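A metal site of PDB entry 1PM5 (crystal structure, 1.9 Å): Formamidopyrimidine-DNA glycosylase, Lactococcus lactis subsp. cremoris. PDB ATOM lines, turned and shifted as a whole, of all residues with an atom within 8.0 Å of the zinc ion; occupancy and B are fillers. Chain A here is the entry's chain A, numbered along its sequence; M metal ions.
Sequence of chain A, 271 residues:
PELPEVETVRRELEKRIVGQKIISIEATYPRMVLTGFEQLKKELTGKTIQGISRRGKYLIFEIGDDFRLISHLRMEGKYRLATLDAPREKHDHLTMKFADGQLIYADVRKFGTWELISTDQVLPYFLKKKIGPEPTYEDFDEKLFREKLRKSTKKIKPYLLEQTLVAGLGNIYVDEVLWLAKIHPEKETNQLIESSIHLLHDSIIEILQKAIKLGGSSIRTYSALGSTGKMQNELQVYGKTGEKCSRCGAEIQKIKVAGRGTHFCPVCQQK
Of the 18 residues printed, 4 come within 4 Å of the zinc ion. The nearest printed residue that does not touch the zinc ion is Val 267 (4.4 Å).
The zinc ion is bound by SG of Cys 265 (2.2 Å), SG of Cys 268 (2.4 Å), SG of Cys 245 (2.4 Å) and SG of Cys 248 (2.5 Å). The zinc ion has four donor atoms within binding distance.
The side-chain sulfur of Cys 268 lies close to the guanidinium group of Arg 247 (3.4 Å). N of Ala 250 lies close to SG of Cys 248 (3.2 Å). The backbone NH of Cys 245 lies within hydrogen-bond range of the backbone carbonyl oxygen of Ala 250 (2.6 Å). N of Cys 265 sits at hydrogen-bond distance from OE1 of Gln 269 (2.9 Å). The side-chain sulfur of Cys 265 sits close to the backbone NH of Val 267 (3.5 Å). The side-chain sulfur (SG) of Cys 245 lies close to the backbone NH (N) of Arg 247, at 3.4 Å. The indole nitrogen (NE1) of Trp 179 lies close to the side-chain sulfur (SG) of Cys 245 (3.4 Å).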
ATOM      1  N   TRP A 179      13.518  -8.784 -22.230  1.00  0.00           N
ATOM      2  CA  TRP A 179      13.042 -10.158 -22.334  1.00  0.00           C
ATOM      3  C   TRP A 179      12.430 -10.545 -20.991  1.00  0.00           C
ATOM      4  O   TRP A 179      11.350 -11.140 -20.937  1.00  0.00           O
ATOM      5  CB  TRP A 179      14.188 -11.128 -22.656  1.00  0.00           C
ATOM      6  CG  TRP A 179      13.761 -12.582 -22.612  1.00  0.00           C
ATOM      7  CD1 TRP A 179      13.204 -13.313 -23.628  1.00  0.00           C
ATOM      8  CD2 TRP A 179      13.830 -13.457 -21.479  1.00  0.00           C
ATOM      9  NE1 TRP A 179      12.931 -14.595 -23.195  1.00  0.00           N
ATOM     10  CE2 TRP A 179      13.304 -14.711 -21.877  1.00  0.00           C
ATOM     11  CE3 TRP A 179      14.295 -13.316 -20.161  1.00  0.00           C
ATOM     12  CZ2 TRP A 179      13.225 -15.812 -21.015  1.00  0.00           C
ATOM     13  CZ3 TRP A 179      14.208 -14.413 -19.294  1.00  0.00           C
ATOM     14  CH2 TRP A 179      13.671 -15.636 -19.735  1.00  0.00           C
ATOM     15  N   LYS A 182       9.187  -8.961 -20.556  1.00  0.00           N
ATOM     16  CA  LYS A 182       8.260  -9.298 -21.632  1.00  0.00           C
ATOM     17  C   LYS A 182       7.789  -8.099 -22.456  1.00  0.00           C
ATOM     18  O   LYS A 182       6.611  -7.943 -22.753  1.00  0.00           O
ATOM     19  CB  LYS A 182       7.038 -10.036 -21.056  1.00  0.00           C
ATOM     20  CG  LYS A 182       7.413 -11.316 -20.326  1.00  0.00           C
ATOM     21  CD  LYS A 182       6.187 -12.059 -19.818  1.00  0.00           C
ATOM     22  CE  LYS A 182       6.589 -13.300 -19.031  1.00  0.00           C
ATOM     23  NZ  LYS A 182       5.396 -14.091 -18.598  1.00  0.00           N
ATOM     24  N   VAL A 237      18.851 -14.087 -23.697  1.00  0.00           N
ATOM     25  CA  VAL A 237      18.640 -13.746 -25.104  1.00  0.00           C
ATOM     26  C   VAL A 237      19.834 -13.165 -25.870  1.00  0.00           C
ATOM     27  O   VAL A 237      20.032 -13.509 -27.035  1.00  0.00           O
ATOM     28  CB  VAL A 237      17.463 -12.758 -25.274  1.00  0.00           C
ATOM     29  CG1 VAL A 237      16.158 -13.441 -24.906  1.00  0.00           C
ATOM     30  CG2 VAL A 237      17.665 -11.524 -24.406  1.00  0.00           C
ATOM     31  N   LYS A 244      16.452 -21.679 -28.299  1.00  0.00           N
ATOM     32  CA  LYS A 244      15.081 -21.617 -27.822  1.00  0.00           C
ATOM     33  C   LYS A 244      14.918 -20.904 -26.486  1.00  0.00           C
ATOM     34  O   LYS A 244      15.686 -21.122 -25.546  1.00  0.00           O
ATOM     35  CB  LYS A 244      14.509 -23.029 -27.757  1.00  0.00           C
ATOM     36  CG  LYS A 244      14.601 -23.761 -29.089  1.00  0.00           C
ATOM     37  CD  LYS A 244      14.038 -25.176 -29.029  1.00  0.00           C
ATOM     38  CE  LYS A 244      14.270 -25.905 -30.343  1.00  0.00           C
ATOM     39  NZ  LYS A 244      13.844 -27.335 -30.316  1.00  0.00           N
ATOM     40  N   CYS A 245      13.901 -20.047 -26.426  1.00  0.00           N
ATOM     41  CA  CYS A 245      13.572 -19.295 -25.232  1.00  0.00           C
ATOM     42  C   CYS A 245      13.358 -20.248 -24.062  1.00  0.00           C
ATOM     43  O   CYS A 245      12.673 -21.260 -24.205  1.00  0.00           O
ATOM     44  CB  CYS A 245      12.305 -18.471 -25.477  1.00  0.00           C
ATOM     45  SG  CYS A 245      11.655 -17.639 -24.036  1.00  0.00           S
ATOM     46  N   SER A 246      13.940 -19.923 -22.914  1.00  0.00           N
ATOM     47  CA  SER A 246      13.828 -20.773 -21.725  1.00  0.00           C
ATOM     48  C   SER A 246      12.439 -20.789 -21.104  1.00  0.00           C
ATOM     49  O   SER A 246      12.162 -21.625 -20.246  1.00  0.00           O
ATOM     50  CB  SER A 246      14.843 -20.334 -20.672  1.00  0.00           C
ATOM     51  OG  SER A 246      14.479 -19.078 -20.110  1.00  0.00           O
ATOM     52  N   ARG A 247      11.580 -19.867 -21.516  1.00  0.00           N
ATOM     53  CA  ARG A 247      10.221 -19.804 -20.976  1.00  0.00           C
ATOM     54  C   ARG A 247       9.166 -20.470 -21.839  1.00  0.00           C
ATOM     55  O   ARG A 247       8.393 -21.283 -21.363  1.00  0.00           O
ATOM     56  CB  ARG A 247       9.799 -18.343 -20.726  1.00  0.00           C
ATOM     57  CG  ARG A 247      10.415 -17.711 -19.504  1.00  0.00           C
ATOM     58  CD  ARG A 247       9.854 -16.323 -19.257  1.00  0.00           C
ATOM     59  NE  ARG A 247       9.994 -15.478 -20.437  1.00  0.00           N
ATOM     60  CZ  ARG A 247      10.168 -14.155 -20.393  1.00  0.00           C
ATOM     61  NH1 ARG A 247      10.226 -13.540 -19.220  1.00  0.00           N
ATOM     62  NH2 ARG A 247      10.285 -13.470 -21.518  1.00  0.00           N
ATOM     63  N   CYS A 248       9.122 -20.100 -23.119  1.00  0.00           N
ATOM     64  CA  CYS A 248       8.109 -20.649 -24.013  1.00  0.00           C
ATOM     65  C   CYS A 248       8.635 -21.651 -25.028  1.00  0.00           C
ATOM     66  O   CYS A 248       7.843 -22.391 -25.623  1.00  0.00           O
ATOM     67  CB  CYS A 248       7.413 -19.515 -24.755  1.00  0.00           C
ATOM     68  SG  CYS A 248       8.394 -18.805 -26.092  1.00  0.00           S
ATOM     69  N   GLY A 249       9.938 -21.666 -25.256  1.00  0.00           N
ATOM     70  CA  GLY A 249      10.510 -22.593 -26.214  1.00  0.00           C
ATOM     71  C   GLY A 249      10.605 -22.087 -27.631  1.00  0.00           C
ATOM     72  O   GLY A 249      11.104 -22.786 -28.501  1.00  0.00           O
ATOM     73  N   ALA A 250      10.127 -20.866 -27.890  1.00  0.00           N
ATOM     74  CA  ALA A 250      10.211 -20.300 -29.227  1.00  0.00           C
ATOM     75  C   ALA A 250      11.658 -19.935 -29.513  1.00  0.00           C
ATOM     76  O   ALA A 250      12.447 -19.743 -28.587  1.00  0.00           O
ATOM     77  CB  ALA A 250       9.329 -19.064 -29.345  1.00  0.00           C
ATOM     78  N   GLU A 251      11.996 -19.837 -30.794  1.00  0.00           N
ATOM     79  CA  GLU A 251      13.358 -19.512 -31.189  1.00  0.00           C
ATOM     80  C   GLU A 251      13.679 -18.022 -31.038  1.00  0.00           C
ATOM     81  O   GLU A 251      12.966 -17.164 -31.534  1.00  0.00           O
ATOM     82  CB  GLU A 251      13.574 -19.929 -32.644  1.00  0.00           C
ATOM     83  CG  GLU A 251      14.991 -20.363 -32.965  1.00  0.00           C
ATOM     84  CD  GLU A 251      15.137 -20.894 -34.376  1.00  0.00           C
ATOM     85  OE1 GLU A 251      15.195 -20.084 -35.325  1.00  0.00           O
ATOM     86  OE2 GLU A 251      15.194 -22.130 -34.534  1.00  0.00           O
ATOM     87  N   ILE A 252      14.768 -17.730 -30.332  1.00  0.00           N
ATOM     88  CA  ILE A 252      15.200 -16.348 -30.138  1.00  0.00           C
ATOM     89  C   ILE A 252      15.595 -15.778 -31.489  1.00  0.00           C
ATOM     90  O   ILE A 252      16.357 -16.397 -32.239  1.00  0.00           O
ATOM     91  CB  ILE A 252      16.403 -16.266 -29.170  1.00  0.00           C
ATOM     92  CG1 ILE A 252      15.999 -16.788 -27.789  1.00  0.00           C
ATOM     93  CG2 ILE A 252      16.919 -14.833 -29.090  1.00  0.00           C
ATOM     94  CD1 ILE A 252      14.791 -16.083 -27.177  1.00  0.00           C
ATOM     95  N   PHE A 264      15.551 -11.050 -29.113  1.00  0.00           N
ATOM     96  CA  PHE A 264      14.298 -11.132 -28.379  1.00  0.00           C
ATOM     97  C   PHE A 264      13.485 -12.383 -28.727  1.00  0.00           C
ATOM     98  O   PHE A 264      13.740 -13.048 -29.737  1.00  0.00           O
ATOM     99  CB  PHE A 264      13.452  -9.894 -28.694  1.00  0.00           C
ATOM    100  CG  PHE A 264      12.820  -9.920 -30.073  1.00  0.00           C
ATOM    101  CD1 PHE A 264      11.492 -10.292 -30.240  1.00  0.00           C
ATOM    102  CD2 PHE A 264      13.586  -9.626 -31.206  1.00  0.00           C
ATOM    103  CE1 PHE A 264      10.925 -10.380 -31.519  1.00  0.00           C
ATOM    104  CE2 PHE A 264      13.035  -9.712 -32.481  1.00  0.00           C
ATOM    105  CZ  PHE A 264      11.699 -10.092 -32.635  1.00  0.00           C
ATOM    106  N   CYS A 265      12.515 -12.713 -27.863  1.00  0.00           N
ATOM    107  CA  CYS A 265      11.620 -13.847 -28.106  1.00  0.00           C
ATOM    108  C   CYS A 265      10.319 -13.263 -28.632  1.00  0.00           C
ATOM    109  O   CYS A 265       9.639 -12.515 -27.916  1.00  0.00           O
ATOM    110  CB  CYS A 265      11.355 -14.619 -26.815  1.00  0.00           C
ATOM    111  SG  CYS A 265      10.023 -15.874 -26.986  1.00  0.00           S
ATOM    112  N   PRO A 266       9.940 -13.600 -29.875  1.00  0.00           N
ATOM    113  CA  PRO A 266       8.721 -13.121 -30.537  1.00  0.00           C
ATOM    114  C   PRO A 266       7.427 -13.498 -29.836  1.00  0.00           C
ATOM    115  O   PRO A 266       6.392 -12.868 -30.038  1.00  0.00           O
ATOM    116  CB  PRO A 266       8.808 -13.735 -31.934  1.00  0.00           C
ATOM    117  CG  PRO A 266      10.282 -13.944 -32.137  1.00  0.00           C
ATOM    118  CD  PRO A 266      10.709 -14.465 -30.790  1.00  0.00           C
ATOM    119  N   VAL A 267       7.466 -14.546 -29.011  1.00  0.00           N
ATOM    120  CA  VAL A 267       6.282 -14.983 -28.287  1.00  0.00           C
ATOM    121  C   VAL A 267       6.159 -14.222 -26.967  1.00  0.00           C
ATOM    122  O   VAL A 267       5.123 -13.615 -26.687  1.00  0.00           O
ATOM    123  CB  VAL A 267       6.335 -16.501 -27.979  1.00  0.00           C
ATOM    124  CG1 VAL A 267       5.176 -16.903 -27.074  1.00  0.00           C
ATOM    125  CG2 VAL A 267       6.276 -17.302 -29.273  1.00  0.00           C
ATOM    126  N   CYS A 268       7.218 -14.248 -26.170  1.00  0.00           N
ATOM    127  CA  CYS A 268       7.232 -13.581 -24.882  1.00  0.00           C
ATOM    128  C   CYS A 268       7.213 -12.057 -24.988  1.00  0.00           C
ATOM    129  O   CYS A 268       6.747 -11.377 -24.070  1.00  0.00           O
ATOM    130  CB  CYS A 268       8.455 -14.012 -24.084  1.00  0.00           C
ATOM    131  SG  CYS A 268       8.391 -15.710 -23.480  1.00  0.00           S
ATOM    132  N   GLN A 269       7.734 -11.532 -26.092  1.00  0.00           N
ATOM    133  CA  GLN A 269       7.795 -10.091 -26.292  1.00  0.00           C
ATOM    134  C   GLN A 269       6.956  -9.675 -27.495  1.00  0.00           C
ATOM    135  O   GLN A 269       7.482  -9.425 -28.590  1.00  0.00           O
ATOM    136  CB  GLN A 269       9.263  -9.674 -26.481  1.00  0.00           C
ATOM    137  CG  GLN A 269      10.108  -9.824 -25.215  1.00  0.00           C
ATOM    138  CD  GLN A 269      11.603  -9.769 -25.476  1.00  0.00           C
ATOM    139  OE1 GLN A 269      12.251 -10.795 -25.714  1.00  0.00           O
ATOM    140  NE2 GLN A 269      12.174  -8.566 -25.452  1.00  0.00           N
HETATM  141 ZN    ZN M   1       9.636 -16.919 -25.072  1.00  0.00          ZN
